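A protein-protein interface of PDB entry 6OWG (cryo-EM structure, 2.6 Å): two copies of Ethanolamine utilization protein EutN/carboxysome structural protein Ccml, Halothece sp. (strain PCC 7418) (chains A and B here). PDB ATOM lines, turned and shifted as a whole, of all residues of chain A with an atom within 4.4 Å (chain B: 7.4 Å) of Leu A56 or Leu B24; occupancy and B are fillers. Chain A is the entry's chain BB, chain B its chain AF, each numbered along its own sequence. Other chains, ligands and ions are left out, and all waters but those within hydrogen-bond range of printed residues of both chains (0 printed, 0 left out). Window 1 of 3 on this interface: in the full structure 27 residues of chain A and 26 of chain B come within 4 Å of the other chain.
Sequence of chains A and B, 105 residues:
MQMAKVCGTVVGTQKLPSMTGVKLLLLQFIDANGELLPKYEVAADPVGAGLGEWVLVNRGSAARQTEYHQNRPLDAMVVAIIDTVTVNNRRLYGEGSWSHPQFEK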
ATOM      1  N   MET A   1      14.552   1.794  16.481  1.00  0.00           N
ATOM      2  CA  MET A   1      13.780   0.957  17.388  1.00  0.00           C
ATOM      3  C   MET A   1      14.666   0.275  18.414  1.00  0.00           C
ATOM      4  O   MET A   1      15.875   0.174  18.245  1.00  0.00           O
ATOM      5  CB  MET A   1      12.994  -0.102  16.613  1.00  0.00           C
ATOM      6  CG  MET A   1      11.669   0.372  16.050  1.00  0.00           C
ATOM      7  SD  MET A   1      11.851   1.411  14.593  1.00  0.00           S
ATOM      8  CE  MET A   1      12.864   0.367  13.553  1.00  0.00           C
ATOM      9  N   GLN A   2      14.042  -0.186  19.488  1.00  0.00           N
ATOM     10  CA  GLN A   2      14.700  -0.977  20.510  1.00  0.00           C
ATOM     11  C   GLN A   2      13.897  -2.245  20.736  1.00  0.00           C
ATOM     12  O   GLN A   2      12.678  -2.262  20.561  1.00  0.00           O
ATOM     13  CB  GLN A   2      14.824  -0.212  21.831  1.00  0.00           C
ATOM     14  CG  GLN A   2      15.847   0.899  21.821  1.00  0.00           C
ATOM     15  CD  GLN A   2      17.259   0.380  21.917  1.00  0.00           C
ATOM     16  OE1 GLN A   2      18.088   0.645  21.052  1.00  0.00           O
ATOM     17  NE2 GLN A   2      17.541  -0.369  22.973  1.00  0.00           N
ATOM     18  N   MET A   3      14.588  -3.309  21.117  1.00  0.00           N
ATOM     19  CA  MET A   3      13.924  -4.529  21.539  1.00  0.00           C
ATOM     20  C   MET A   3      13.598  -4.425  23.019  1.00  0.00           C
ATOM     21  O   MET A   3      14.438  -4.020  23.825  1.00  0.00           O
ATOM     22  CB  MET A   3      14.801  -5.751  21.275  1.00  0.00           C
ATOM     23  CG  MET A   3      15.119  -5.974  19.814  1.00  0.00           C
ATOM     24  SD  MET A   3      15.762  -7.618  19.490  1.00  0.00           S
ATOM     25  CE  MET A   3      17.224  -7.618  20.515  1.00  0.00           C
ATOM     26  N   VAL A  55       8.954  -7.082  21.989  1.00  0.00           N
ATOM     27  CA  VAL A  55       8.365  -6.081  21.116  1.00  0.00           C
ATOM     28  C   VAL A  55       9.458  -5.169  20.584  1.00  0.00           C
ATOM     29  O   VAL A  55      10.534  -5.036  21.167  1.00  0.00           O
ATOM     30  CB  VAL A  55       7.276  -5.248  21.829  1.00  0.00           C
ATOM     31  CG1 VAL A  55       6.044  -6.090  22.091  1.00  0.00           C
ATOM     32  CG2 VAL A  55       7.808  -4.653  23.118  1.00  0.00           C
ATOM     33  N   LEU A  56       9.168  -4.550  19.447  1.00  0.00           N
ATOM     34  CA  LEU A  56       9.962  -3.446  18.931  1.00  0.00           C
ATOM     35  C   LEU A  56       9.263  -2.152  19.307  1.00  0.00           C
ATOM     36  O   LEU A  56       8.082  -1.970  18.998  1.00  0.00           O
ATOM     37  CB  LEU A  56      10.139  -3.533  17.418  1.00  0.00           C
ATOM     38  CG  LEU A  56      11.261  -4.410  16.872  1.00  0.00           C
ATOM     39  CD1 LEU A  56      11.433  -4.123  15.404  1.00  0.00           C
ATOM     40  CD2 LEU A  56      12.560  -4.178  17.617  1.00  0.00           C
ATOM     41  N   VAL A  57       9.982  -1.264  19.976  1.00  0.00           N
ATOM     42  CA  VAL A  57       9.439   0.009  20.417  1.00  0.00           C
ATOM     43  C   VAL A  57      10.303   1.133  19.858  1.00  0.00           C
ATOM     44  O   VAL A  57      11.535   1.066  19.892  1.00  0.00           O
ATOM     45  CB  VAL A  57       9.308   0.055  21.960  1.00  0.00           C
ATOM     46  CG1 VAL A  57      10.618  -0.260  22.660  1.00  0.00           C
ATOM     47  CG2 VAL A  57       8.765   1.392  22.426  1.00  0.00           C
ATOM     48  N   ASN A  58       9.656   2.129  19.268  1.00  0.00           N
ATOM     49  CA  ASN A  58      10.359   3.307  18.804  1.00  0.00           C
ATOM     50  C   ASN A  58      10.186   4.428  19.822  1.00  0.00           C
ATOM     51  O   ASN A  58       9.463   4.293  20.810  1.00  0.00           O
ATOM     52  CB  ASN A  58       9.895   3.703  17.396  1.00  0.00           C
ATOM     53  CG  ASN A  58       8.402   4.001  17.303  1.00  0.00           C
ATOM     54  OD1 ASN A  58       7.662   3.959  18.277  1.00  0.00           O
ATOM     55  ND2 ASN A  58       7.961   4.304  16.100  1.00  0.00           N
ATOM     56  N   MET A  77       6.132   3.913  21.362  1.00  0.00           N
ATOM     57  CA  MET A  77       5.062   3.127  20.768  1.00  0.00           C
ATOM     58  C   MET A  77       5.609   1.767  20.376  1.00  0.00           C
ATOM     59  O   MET A  77       6.662   1.685  19.743  1.00  0.00           O
ATOM     60  CB  MET A  77       4.477   3.840  19.547  1.00  0.00           C
ATOM     61  CG  MET A  77       3.521   3.011  18.727  1.00  0.00           C
ATOM     62  SD  MET A  77       2.438   4.018  17.709  1.00  0.00           S
ATOM     63  CE  MET A  77       3.449   4.236  16.258  1.00  0.00           C
ATOM     64  N   VAL A  78       4.904   0.708  20.760  1.00  0.00           N
ATOM     65  CA  VAL A  78       5.207  -0.617  20.236  1.00  0.00           C
ATOM     66  C   VAL A  78       4.778  -0.661  18.776  1.00  0.00           C
ATOM     67  O   VAL A  78       3.603  -0.457  18.453  1.00  0.00           O
ATOM     68  CB  VAL A  78       4.509  -1.706  21.057  1.00  0.00           C
ATOM     69  CG1 VAL A  78       4.598  -3.040  20.349  1.00  0.00           C
ATOM     70  CG2 VAL A  78       5.116  -1.791  22.438  1.00  0.00           C
ATOM     71  N   VAL A  79       5.733  -0.908  17.884  1.00  0.00           N
ATOM     72  CA  VAL A  79       5.440  -0.948  16.458  1.00  0.00           C
ATOM     73  C   VAL A  79       5.354  -2.369  15.919  1.00  0.00           C
ATOM     74  O   VAL A  79       4.736  -2.580  14.865  1.00  0.00           O
ATOM     75  CB  VAL A  79       6.481  -0.139  15.656  1.00  0.00           C
ATOM     76  CG1 VAL A  79       6.350   1.325  15.973  1.00  0.00           C
ATOM     77  CG2 VAL A  79       7.887  -0.620  15.949  1.00  0.00           C
ATOM     78  N   ALA A  80       5.935  -3.343  16.608  1.00  0.00           N
ATOM     79  CA  ALA A  80       5.956  -4.711  16.127  1.00  0.00           C
ATOM     80  C   ALA A  80       6.098  -5.644  17.312  1.00  0.00           C
ATOM     81  O   ALA A  80       6.726  -5.303  18.314  1.00  0.00           O
ATOM     82  CB  ALA A  80       7.102  -4.941  15.141  1.00  0.00           C
ATOM     83  N   ILE A  82       7.936  -9.048  18.123  1.00  0.00           N
ATOM     84  CA  ILE A  82       9.081  -9.728  17.536  1.00  0.00           C
ATOM     85  C   ILE A  82       8.758 -11.207  17.376  1.00  0.00           C
ATOM     86  O   ILE A  82       8.380 -11.885  18.337  1.00  0.00           O
ATOM     87  CB  ILE A  82      10.335  -9.515  18.393  1.00  0.00           C
ATOM     88  CG1 ILE A  82      10.875  -8.101  18.203  1.00  0.00           C
ATOM     89  CG2 ILE A  82      11.397 -10.522  18.046  1.00  0.00           C
ATOM     90  CD1 ILE A  82      11.843  -7.687  19.268  1.00  0.00           C
ATOM     91  N   GLY B   8      22.750  -8.670  13.059  1.00  0.00           N
ATOM     92  CA  GLY B   8      21.709  -9.610  12.734  1.00  0.00           C
ATOM     93  C   GLY B   8      20.458  -8.951  12.207  1.00  0.00           C
ATOM     94  O   GLY B   8      20.448  -7.769  11.865  1.00  0.00           O
ATOM     95  N   THR B   9      19.394  -9.749  12.139  1.00  0.00           N
ATOM     96  CA  THR B   9      18.110  -9.328  11.604  1.00  0.00           C
ATOM     97  C   THR B   9      17.028  -9.548  12.648  1.00  0.00           C
ATOM     98  O   THR B   9      17.109 -10.478  13.453  1.00  0.00           O
ATOM     99  CB  THR B   9      17.739 -10.098  10.321  1.00  0.00           C
ATOM    100  OG1 THR B   9      17.661 -11.500  10.604  1.00  0.00           O
ATOM    101  CG2 THR B   9      18.764  -9.870   9.232  1.00  0.00           C
ATOM    102  N   VAL B  10      16.021  -8.681  12.633  1.00  0.00           N
ATOM    103  CA  VAL B  10      14.843  -8.808  13.480  1.00  0.00           C
ATOM    104  C   VAL B  10      13.633  -8.956  12.573  1.00  0.00           C
ATOM    105  O   VAL B  10      13.370  -8.088  11.734  1.00  0.00           O
ATOM    106  CB  VAL B  10      14.681  -7.600  14.419  1.00  0.00           C
ATOM    107  CG1 VAL B  10      13.443  -7.760  15.277  1.00  0.00           C
ATOM    108  CG2 VAL B  10      15.910  -7.430  15.288  1.00  0.00           C
ATOM    109  N   VAL B  11      12.903 -10.052  12.735  1.00  0.00           N
ATOM    110  CA  VAL B  11      11.703 -10.321  11.955  1.00  0.00           C
ATOM    111  C   VAL B  11      10.513 -10.262  12.898  1.00  0.00           C
ATOM    112  O   VAL B  11      10.487 -10.961  13.917  1.00  0.00           O
ATOM    113  CB  VAL B  11      11.779 -11.680  11.240  1.00  0.00           C
ATOM    114  CG1 VAL B  11      10.415 -12.098  10.725  1.00  0.00           C
ATOM    115  CG2 VAL B  11      12.776 -11.618  10.098  1.00  0.00           C
ATOM    116  N   GLY B  12       9.546  -9.413  12.575  1.00  0.00           N
ATOM    117  CA  GLY B  12       8.289  -9.387  13.290  1.00  0.00           C
ATOM    118  C   GLY B  12       7.123  -9.527  12.339  1.00  0.00           C
ATOM    119  O   GLY B  12       7.008  -8.756  11.386  1.00  0.00           O
ATOM    120  N   LYS B  15       2.720  -6.749  13.349  1.00  0.00           N
ATOM    121  CA  LYS B  15       3.265  -5.400  13.380  1.00  0.00           C
ATOM    122  C   LYS B  15       2.200  -4.429  12.891  1.00  0.00           C
ATOM    123  O   LYS B  15       1.061  -4.809  12.615  1.00  0.00           O
ATOM    124  CB  LYS B  15       4.530  -5.303  12.528  1.00  0.00           C
ATOM    125  CG  LYS B  15       4.387  -5.896  11.147  1.00  0.00           C
ATOM    126  CD  LYS B  15       5.704  -5.882  10.411  1.00  0.00           C
ATOM    127  CE  LYS B  15       5.626  -6.689   9.133  1.00  0.00           C
ATOM    128  NZ  LYS B  15       6.908  -6.636   8.382  1.00  0.00           N
ATOM    129  N   MET B  19       4.402  -0.727   8.884  1.00  0.00           N
ATOM    130  CA  MET B  19       5.724  -1.298   9.098  1.00  0.00           C
ATOM    131  C   MET B  19       6.033  -2.460   8.163  1.00  0.00           C
ATOM    132  O   MET B  19       7.065  -3.112   8.346  1.00  0.00           O
ATOM    133  CB  MET B  19       5.867  -1.763  10.546  1.00  0.00           C
ATOM    134  CG  MET B  19       6.156  -0.651  11.531  1.00  0.00           C
ATOM    135  SD  MET B  19       7.701   0.207  11.183  1.00  0.00           S
ATOM    136  CE  MET B  19       8.884  -1.095  11.512  1.00  0.00           C
ATOM    137  N   GLY B  21       7.147  -4.377   4.649  1.00  0.00           N
ATOM    138  CA  GLY B  21       8.162  -4.083   3.664  1.00  0.00           C
ATOM    139  C   GLY B  21       9.432  -3.473   4.213  1.00  0.00           C
ATOM    140  O   GLY B  21      10.393  -3.299   3.454  1.00  0.00           O
ATOM    141  N   VAL B  22       9.474  -3.151   5.502  1.00  0.00           N
ATOM    142  CA  VAL B  22      10.620  -2.513   6.132  1.00  0.00           C
ATOM    143  C   VAL B  22      11.560  -3.603   6.623  1.00  0.00           C
ATOM    144  O   VAL B  22      11.185  -4.426   7.466  1.00  0.00           O
ATOM    145  CB  VAL B  22      10.183  -1.597   7.286  1.00  0.00           C
ATOM    146  CG1 VAL B  22      11.387  -1.076   8.037  1.00  0.00           C
ATOM    147  CG2 VAL B  22       9.342  -0.449   6.763  1.00  0.00           C
ATOM    148  N   LYS B  23      12.777  -3.614   6.092  1.00  0.00           N
ATOM    149  CA  LYS B  23      13.795  -4.560   6.521  1.00  0.00           C
ATOM    150  C   LYS B  23      14.448  -4.039   7.793  1.00  0.00           C
ATOM    151  O   LYS B  23      14.916  -2.898   7.833  1.00  0.00           O
ATOM    152  CB  LYS B  23      14.823  -4.760   5.411  1.00  0.00           C
ATOM    153  CG  LYS B  23      16.085  -5.478   5.830  1.00  0.00           C
ATOM    154  CD  LYS B  23      17.146  -5.344   4.754  1.00  0.00           C
ATOM    155  CE  LYS B  23      18.462  -5.946   5.195  1.00  0.00           C
ATOM    156  NZ  LYS B  23      19.577  -5.548   4.297  1.00  0.00           N
ATOM    157  N   LEU B  24      14.474  -4.867   8.831  1.00  0.00           N
ATOM    158  CA  LEU B  24      14.924  -4.462  10.154  1.00  0.00           C
ATOM    159  C   LEU B  24      16.218  -5.176  10.506  1.00  0.00           C
ATOM    160  O   LEU B  24      16.247  -6.404  10.606  1.00  0.00           O
ATOM    161  CB  LEU B  24      13.856  -4.765  11.204  1.00  0.00           C
ATOM    162  CG  LEU B  24      12.509  -4.102  10.944  1.00  0.00           C
ATOM    163  CD1 LEU B  24      11.425  -4.797  11.729  1.00  0.00           C
ATOM    164  CD2 LEU B  24      12.576  -2.634  11.295  1.00  0.00           C
ATOM    165  N   LEU B  25      17.279  -4.405  10.693  1.00  0.00           N
ATOM    166  CA  LEU B  25      18.587  -4.937  11.030  1.00  0.00           C
ATOM    167  C   LEU B  25      18.907  -4.665  12.491  1.00  0.00           C
ATOM    168  O   LEU B  25      18.672  -3.576  13.012  1.00  0.00           O
ATOM    169  CB  LEU B  25      19.668  -4.324  10.136  1.00  0.00           C
ATOM    170  CG  LEU B  25      19.735  -4.803   8.692  1.00  0.00           C
ATOM    171  CD1 LEU B  25      20.932  -4.190   8.020  1.00  0.00           C
ATOM    172  CD2 LEU B  25      19.818  -6.308   8.647  1.00  0.00           C
ATOM    173  N   LEU B  26      19.463  -5.674  13.148  1.00  0.00           N
ATOM    174  CA  LEU B  26      20.001  -5.534  14.493  1.00  0.00           C
ATOM    175  C   LEU B  26      21.438  -5.048  14.361  1.00  0.00           C
ATOM    176  O   LEU B  26      22.308  -5.789  13.895  1.00  0.00           O
ATOM    177  CB  LEU B  26      19.929  -6.852  15.257  1.00  0.00           C
ATOM    178  CG  LEU B  26      20.396  -6.780  16.707  1.00  0.00           C
ATOM    179  CD1 LEU B  26      19.307  -6.198  17.575  1.00  0.00           C
ATOM    180  CD2 LEU B  26      20.804  -8.149  17.200  1.00  0.00           C
ATOM    181  N   LEU B  27      21.682  -3.806  14.758  1.00  0.00           N
ATOM    182  CA  LEU B  27      22.989  -3.178  14.643  1.00  0.00           C
ATOM    183  C   LEU B  27      23.570  -2.963  16.027  1.00  0.00           C
ATOM    184  O   LEU B  27      22.892  -2.426  16.901  1.00  0.00           O
ATOM    185  CB  LEU B  27      22.893  -1.832  13.929  1.00  0.00           C
ATOM    186  CG  LEU B  27      21.984  -1.686  12.721  1.00  0.00           C
ATOM    187  CD1 LEU B  27      21.855  -0.230  12.398  1.00  0.00           C
ATOM    188  CD2 LEU B  27      22.561  -2.433  11.551  1.00  0.00           C
ATOM    189  N   TYR B  40      22.885  -1.193  21.285  1.00  0.00           N
ATOM    190  CA  TYR B  40      22.394  -1.659  20.002  1.00  0.00           C
ATOM    191  C   TYR B  40      21.273  -0.764  19.497  1.00  0.00           C
ATOM    192  O   TYR B  40      20.866   0.198  20.151  1.00  0.00           O
ATOM    193  CB  TYR B  40      21.897  -3.109  20.085  1.00  0.00           C
ATOM    194  CG  TYR B  40      20.562  -3.248  20.770  1.00  0.00           C
ATOM    195  CD1 TYR B  40      20.458  -3.102  22.143  1.00  0.00           C
ATOM    196  CD2 TYR B  40      19.404  -3.528  20.047  1.00  0.00           C
ATOM    197  CE1 TYR B  40      19.260  -3.210  22.774  1.00  0.00           C
ATOM    198  CE2 TYR B  40      18.187  -3.644  20.678  1.00  0.00           C
ATOM    199  CZ  TYR B  40      18.126  -3.485  22.045  1.00  0.00           C
ATOM    200  OH  TYR B  40      16.931  -3.600  22.710  1.00  0.00           O
ATOM    201  N   GLU B  41      20.780  -1.108  18.312  1.00  0.00           N
ATOM    202  CA  GLU B  41      19.658  -0.435  17.682  1.00  0.00           C
ATOM    203  C   GLU B  41      19.036  -1.388  16.675  1.00  0.00           C
ATOM    204  O   GLU B  41      19.704  -2.281  16.150  1.00  0.00           O
ATOM    205  CB  GLU B  41      20.099   0.861  16.986  1.00  0.00           C
ATOM    206  CG  GLU B  41      19.003   1.891  16.778  1.00  0.00           C
ATOM    207  CD  GLU B  41      18.641   2.643  18.045  1.00  0.00           C
ATOM    208  OE1 GLU B  41      19.555   2.972  18.830  1.00  0.00           O
ATOM    209  OE2 GLU B  41      17.438   2.909  18.254  1.00  0.00           O
ATOM    210  N   VAL B  42      17.745  -1.209  16.424  1.00  0.00           N
ATOM    211  CA  VAL B  42      17.063  -1.855  15.311  1.00  0.00           C
ATOM    212  C   VAL B  42      16.686  -0.755  14.333  1.00  0.00           C
ATOM    213  O   VAL B  42      15.986   0.194  14.698  1.00  0.00           O
ATOM    214  CB  VAL B  42      15.832  -2.651  15.770  1.00  0.00           C
ATOM    215  CG1 VAL B  42      15.191  -3.352  14.589  1.00  0.00           C
ATOM    216  CG2 VAL B  42      16.225  -3.656  16.831  1.00  0.00           C
ATOM    217  N   ALA B  43      17.161  -0.869  13.099  1.00  0.00           N
ATOM    218  CA  ALA B  43      17.013   0.200  12.129  1.00  0.00           C
ATOM    219  C   ALA B  43      16.425  -0.326  10.832  1.00  0.00           C
ATOM    220  O   ALA B  43      16.608  -1.489  10.472  1.00  0.00           O
ATOM    221  CB  ALA B  43      18.350   0.874  11.840  1.00  0.00           C
ATOM    222  N   ALA B  44      15.704   0.551  10.143  1.00  0.00           N
ATOM    223  CA  ALA B  44      15.301   0.291   8.773  1.00  0.00           C
ATOM    224  C   ALA B  44      16.518   0.339   7.861  1.00  0.00           C
ATOM    225  O   ALA B  44      17.465   1.093   8.090  1.00  0.00           O
ATOM    226  CB  ALA B  44      14.264   1.314   8.321  1.00  0.00           C
ATOM    227  N   ASP B  45      16.492  -0.477   6.809  1.00  0.00           N
ATOM    228  CA  ASP B  45      17.647  -0.665   5.935  1.00  0.00           C
ATOM    229  C   ASP B  45      17.249  -0.448   4.478  1.00  0.00           C
ATOM    230  O   ASP B  45      16.938  -1.409   3.760  1.00  0.00           O
ATOM    231  CB  ASP B  45      18.245  -2.053   6.141  1.00  0.00           C
ATOM    232  CG  ASP B  45      19.541  -2.238   5.406  1.00  0.00           C
ATOM    233  OD1 ASP B  45      20.562  -1.699   5.870  1.00  0.00           O
ATOM    234  OD2 ASP B  45      19.545  -2.926   4.368  1.00  0.00           O
ATOM    235  N   LEU B  74       9.305   5.051  12.278  1.00  0.00           N
ATOM    236  CA  LEU B  74      10.707   4.660  12.296  1.00  0.00           C
ATOM    237  C   LEU B  74      11.528   5.739  12.984  1.00  0.00           C
ATOM    238  O   LEU B  74      11.352   6.928  12.706  1.00  0.00           O
ATOM    239  CB  LEU B  74      11.223   4.430  10.876  1.00  0.00           C
ATOM    240  CG  LEU B  74      10.565   3.276  10.127  1.00  0.00           C
ATOM    241  CD1 LEU B  74      10.942   3.318   8.672  1.00  0.00           C
ATOM    242  CD2 LEU B  74      10.974   1.960  10.738  1.00  0.00           C
ATOM    243  N   ALA B  76      15.089   4.969  13.454  1.00  0.00           N
ATOM    244  CA  ALA B  76      16.456   4.565  13.171  1.00  0.00           C
ATOM    245  C   ALA B  76      16.504   4.032  11.751  1.00  0.00           C
ATOM    246  O   ALA B  76      15.612   3.291  11.335  1.00  0.00           O
ATOM    247  CB  ALA B  76      16.949   3.502  14.155  1.00  0.00           C
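CE of Met A1 touches CD2 of Leu B24, at 3.8 Å. CE of Met A1 touches CD2 of Leu B74, 3.7 Å away. N of Met A1 touches CB of Ala B76, 3.8 Å away. Gln A2 touches Glu B41. Met A3 touches Val B42 (CG to CG2, 3.9 Å). Leu A56 touches Leu B24. Lys B15 touches Val A79 (CA to O, 3.5 Å). CB of Ala A80 touches CB of Lys B15, at 3.7 Å. CG1 of Ile A82 touches CG1 of Val B10, 3.9 Å away. Ile A82 touches Val B11 (C to O, 3.9 Å).
O of Gly B8 lies within hydrogen-bond range of N of Leu B26. The backbone NH of Val B10 lies within hydrogen-bond range of the backbone carbonyl oxygen of Leu B24 (3.1 Å). The backbone NH (N) of Leu B27 sits at hydrogen-bond distance from the backbone carbonyl oxygen (O) of Glu B41, 2.9 Å away. The backbone NH (N) of Ala B44 sits at hydrogen-bond distance from the backbone carbonyl oxygen (O) of Ala B76 (3.0 Å). N of Gln A2 sits at hydrogen-bond distance from O of Val A57 (2.8 Å). O of Leu A56 sits at hydrogen-bond distance from N of Val A79, 2.8 Å away.
Of the printed residues of chain B, Met A1 touches Leu B24, Glu B41, Val B42, Leu B74 and Ala B76. Of the printed residues of chain B, Met A3 touches Leu B26 (3.9 Å), Tyr B40 (2.8 Å) and Val B42 (3.9 Å). Of chain B, only Leu B24 (3.7 Å) and Val B42 (3.8 Å) come within 4 Å of Leu A56. Of the printed residues of chain B, Ala A80 touches Lys B15. Met B19 touches none of the printed residues of chain A. Of chain A, only Met A1 and Leu A56 come within 4 Å of Leu B24. The nearest residue of chain B that does not touch Leu A56 is Val B10 (4.2 Å). The nearest printed residue of chain A that does not touch Leu B24 is Ala A80 (5.5 Å).
The backbone carbonyl oxygen (O) of Tyr B40 sits close to the side-chain amide oxygen (OE1) of Gln A2 (3.0 Å). The side-chain hydroxyl (OH) of Tyr B40 is in hydrogen-bond range of the backbone carbonyl oxygen (O) of Met A3 (2.8 Å). The backbone carbonyl oxygen of Val B42 is in hydrogen-bond range of the backbone NH of Met A1 (2.8 Å). The backbone carbonyl oxygen of Met A1 sits close to the side-chain carboxylate of Glu B41 (3.2 Å).
No position is printed for both chains.
Of the 22 printed residues of chain B, 10 touch a printed residue of chain A. Hydrophobic or aromatic side chains of chain B that line the printed part of chain A: Val B10, Leu B24, Leu B26, Tyr B40, Val B42, Leu B74 and Ala B76. Among the printed residues, no Asp or Glu carboxylate lies within 4 Å of a Lys or Arg side-chain nitrogen of the other chain.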
